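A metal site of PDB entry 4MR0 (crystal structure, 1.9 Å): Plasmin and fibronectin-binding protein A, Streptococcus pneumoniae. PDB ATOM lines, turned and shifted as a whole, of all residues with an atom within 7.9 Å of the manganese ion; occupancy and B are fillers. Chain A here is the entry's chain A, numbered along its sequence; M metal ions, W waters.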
ATOM      1  N   LYS A 161      11.492 -18.231 -26.096  1.00  0.00           N
ATOM      2  CA  LYS A 161      11.250 -19.503 -25.440  1.00  0.00           C
ATOM      3  C   LYS A 161      12.525 -20.222 -25.016  1.00  0.00           C
ATOM      4  O   LYS A 161      12.483 -21.348 -24.505  1.00  0.00           O
ATOM      5  CB  LYS A 161      10.399 -20.414 -26.330  1.00  0.00           C
ATOM      6  CG  LYS A 161       8.976 -19.910 -26.525  1.00  0.00           C
ATOM      7  CD  LYS A 161       8.070 -21.037 -26.967  1.00  0.00           C
ATOM      8  CE  LYS A 161       6.647 -20.561 -27.187  1.00  0.00           C
ATOM      9  NZ  LYS A 161       5.747 -21.728 -27.472  1.00  0.00           N
ATOM     10  N   GLU A 162      13.662 -19.565 -25.249  1.00  0.00           N
ATOM     11  CA  GLU A 162      14.960 -20.090 -24.850  1.00  0.00           C
ATOM     12  C   GLU A 162      15.880 -18.893 -24.614  1.00  0.00           C
ATOM     13  O   GLU A 162      15.539 -17.752 -24.947  1.00  0.00           O
ATOM     14  CB  GLU A 162      15.557 -21.017 -25.915  1.00  0.00           C
ATOM     15  CG  GLU A 162      15.651 -22.497 -25.496  1.00  0.00           C
ATOM     16  CD  GLU A 162      16.764 -22.795 -24.491  1.00  0.00           C
ATOM     17  OE1 GLU A 162      17.495 -21.867 -24.072  1.00  0.00           O
ATOM     18  OE2 GLU A 162      16.933 -23.982 -24.124  1.00  0.00           O
ATOM     19  N   ILE A 163      17.048 -19.177 -24.034  1.00  0.00           N
ATOM     20  CA  ILE A 163      18.040 -18.167 -23.707  1.00  0.00           C
ATOM     21  C   ILE A 163      18.684 -17.502 -24.908  1.00  0.00           C
ATOM     22  O   ILE A 163      18.993 -18.160 -25.902  1.00  0.00           O
ATOM     23  CB  ILE A 163      19.174 -18.802 -22.848  1.00  0.00           C
ATOM     24  CG1 ILE A 163      18.572 -19.482 -21.607  1.00  0.00           C
ATOM     25  CG2 ILE A 163      20.200 -17.745 -22.445  1.00  0.00           C
ATOM     26  CD1 ILE A 163      19.572 -20.350 -20.849  1.00  0.00           C
ATOM     27  N   PHE A 165      21.910 -15.301 -26.276  1.00  0.00           N
ATOM     28  CA  PHE A 165      23.304 -15.124 -25.898  1.00  0.00           C
ATOM     29  C   PHE A 165      23.924 -13.858 -26.438  1.00  0.00           C
ATOM     30  O   PHE A 165      24.011 -13.664 -27.656  1.00  0.00           O
ATOM     31  CB  PHE A 165      24.090 -16.349 -26.358  1.00  0.00           C
ATOM     32  CG  PHE A 165      23.521 -17.639 -25.850  1.00  0.00           C
ATOM     33  CD1 PHE A 165      23.641 -17.976 -24.497  1.00  0.00           C
ATOM     34  CD2 PHE A 165      22.815 -18.485 -26.694  1.00  0.00           C
ATOM     35  CE1 PHE A 165      23.044 -19.130 -24.005  1.00  0.00           C
ATOM     36  CE2 PHE A 165      22.208 -19.649 -26.200  1.00  0.00           C
ATOM     37  CZ  PHE A 165      22.326 -19.975 -24.856  1.00  0.00           C
ATOM     38  N   ILE A 184      10.710 -18.642 -21.249  1.00  0.00           N
ATOM     39  CA  ILE A 184      11.542 -19.803 -20.975  1.00  0.00           C
ATOM     40  C   ILE A 184      10.916 -20.603 -19.835  1.00  0.00           C
ATOM     41  O   ILE A 184      11.035 -20.240 -18.666  1.00  0.00           O
ATOM     42  CB  ILE A 184      12.972 -19.367 -20.611  1.00  0.00           C
ATOM     43  CG1 ILE A 184      13.485 -18.368 -21.653  1.00  0.00           C
ATOM     44  CG2 ILE A 184      13.902 -20.574 -20.572  1.00  0.00           C
ATOM     45  CD1 ILE A 184      14.750 -17.633 -21.236  1.00  0.00           C
ATOM     46  N   ILE A 186      11.277 -24.264 -18.941  1.00  0.00           N
ATOM     47  CA  ILE A 186      11.914 -25.567 -19.078  1.00  0.00           C
ATOM     48  C   ILE A 186      12.251 -26.193 -17.720  1.00  0.00           C
ATOM     49  O   ILE A 186      12.812 -25.542 -16.845  1.00  0.00           O
ATOM     50  CB  ILE A 186      13.198 -25.413 -19.936  1.00  0.00           C
ATOM     51  CG1 ILE A 186      12.849 -24.770 -21.280  1.00  0.00           C
ATOM     52  CG2 ILE A 186      13.851 -26.761 -20.168  1.00  0.00           C
ATOM     53  CD1 ILE A 186      14.054 -24.391 -22.120  1.00  0.00           C
ATOM     54  N   HIS A 189      15.880 -26.376 -15.577  1.00  0.00           N
ATOM     55  CA  HIS A 189      16.603 -25.477 -16.476  1.00  0.00           C
ATOM     56  C   HIS A 189      16.409 -24.019 -16.046  1.00  0.00           C
ATOM     57  O   HIS A 189      15.344 -23.632 -15.552  1.00  0.00           O
ATOM     58  CB  HIS A 189      16.025 -25.713 -17.886  1.00  0.00           C
ATOM     59  CG  HIS A 189      16.772 -25.032 -19.000  1.00  0.00           C
ATOM     60  ND1 HIS A 189      16.767 -23.662 -19.175  1.00  0.00           N
ATOM     61  CD2 HIS A 189      17.457 -25.544 -20.044  1.00  0.00           C
ATOM     62  CE1 HIS A 189      17.413 -23.367 -20.292  1.00  0.00           C
ATOM     63  NE2 HIS A 189      17.838 -24.490 -20.841  1.00  0.00           N
ATOM     64  N   PRO A 190      17.456 -23.185 -16.202  1.00  0.00           N
ATOM     65  CA  PRO A 190      17.301 -21.786 -15.789  1.00  0.00           C
ATOM     66  C   PRO A 190      16.310 -21.037 -16.667  1.00  0.00           C
ATOM     67  O   PRO A 190      16.055 -21.415 -17.819  1.00  0.00           O
ATOM     68  CB  PRO A 190      18.722 -21.233 -15.902  1.00  0.00           C
ATOM     69  CG  PRO A 190      19.360 -22.096 -16.953  1.00  0.00           C
ATOM     70  CD  PRO A 190      18.836 -23.474 -16.617  1.00  0.00           C
ATOM     71  N   PHE A 199      24.738 -22.050 -22.984  1.00  0.00           N
ATOM     72  CA  PHE A 199      24.104 -22.960 -22.042  1.00  0.00           C
ATOM     73  C   PHE A 199      23.090 -23.772 -22.843  1.00  0.00           C
ATOM     74  O   PHE A 199      22.365 -23.225 -23.677  1.00  0.00           O
ATOM     75  CB  PHE A 199      23.381 -22.209 -20.915  1.00  0.00           C
ATOM     76  CG  PHE A 199      22.781 -23.112 -19.878  1.00  0.00           C
ATOM     77  CD1 PHE A 199      21.554 -23.736 -20.093  1.00  0.00           C
ATOM     78  CD2 PHE A 199      23.483 -23.408 -18.705  1.00  0.00           C
ATOM     79  CE1 PHE A 199      21.033 -24.640 -19.172  1.00  0.00           C
ATOM     80  CE2 PHE A 199      22.975 -24.314 -17.778  1.00  0.00           C
ATOM     81  CZ  PHE A 199      21.746 -24.940 -18.007  1.00  0.00           C
ATOM     82  N   THR A 200      23.054 -25.081 -22.615  1.00  0.00           N
ATOM     83  CA  THR A 200      22.131 -25.967 -23.314  1.00  0.00           C
ATOM     84  C   THR A 200      21.252 -26.648 -22.271  1.00  0.00           C
ATOM     85  O   THR A 200      20.087 -26.299 -22.091  1.00  0.00           O
ATOM     86  CB  THR A 200      22.890 -27.032 -24.132  1.00  0.00           C
ATOM     87  OG1 THR A 200      23.885 -27.660 -23.309  1.00  0.00           O
ATOM     88  CG2 THR A 200      23.573 -26.399 -25.325  1.00  0.00           C
ATOM     89  N   ASP A 201      21.816 -27.641 -21.583  1.00  0.00           N
ATOM     90  CA  ASP A 201      21.073 -28.349 -20.551  1.00  0.00           C
ATOM     91  C   ASP A 201      22.000 -28.631 -19.384  1.00  0.00           C
ATOM     92  O   ASP A 201      23.232 -28.611 -19.526  1.00  0.00           O
ATOM     93  CB  ASP A 201      20.519 -29.663 -21.091  1.00  0.00           C
ATOM     94  CG  ASP A 201      19.672 -29.473 -22.341  1.00  0.00           C
ATOM     95  OD1 ASP A 201      20.233 -29.482 -23.453  1.00  0.00           O
ATOM     96  OD2 ASP A 201      18.442 -29.292 -22.207  1.00  0.00           O
ATOM     97  N   ASP A 202      21.428 -28.885 -18.209  1.00  0.00           N
ATOM     98  CA  ASP A 202      22.240 -29.176 -17.035  1.00  0.00           C
ATOM     99  C   ASP A 202      22.990 -30.477 -17.292  1.00  0.00           C
ATOM    100  O   ASP A 202      22.424 -31.438 -17.818  1.00  0.00           O
ATOM    101  CB  ASP A 202      21.338 -29.292 -15.808  1.00  0.00           C
ATOM    102  CG  ASP A 202      22.126 -29.424 -14.517  1.00  0.00           C
ATOM    103  OD1 ASP A 202      23.221 -28.816 -14.429  1.00  0.00           O
ATOM    104  OD2 ASP A 202      21.659 -30.119 -13.598  1.00  0.00           O
HETATM  105 MN    MN M   1      18.473 -25.061 -23.008  1.00  0.00          MN
HETATM  106  O   HOH W   1      19.751 -23.075 -23.319  1.00  0.00           O
HETATM  107  O   HOH W   2      17.074 -26.985 -23.052  1.00  0.00           O
HETATM  108  O   HOH W   3      19.306 -25.530 -25.060  1.00  0.00           O
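OE2 of Glu 162 is bound to the manganese ion (2.2 Å). The manganese ion is bound by the backbone carbonyl oxygen (O) of Thr 200, at 2.2 Å. The manganese ion is bound by water W3, 2.3 Å away. A ring nitrogen (NE2) of His 189 binds the manganese ion, at 2.3 Å. Water W2 is bound to the manganese ion, at 2.4 Å. Water W1 is bound to the manganese ion (2.4 Å).
Within 4 Å of the manganese ion: Glu 162, His 189 and Thr 200.
Water W1 lies within hydrogen-bond range of the backbone carbonyl oxygen of Phe 199 (2.6 Å) and the side-chain carboxylate of Glu 162 (2.7 Å).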
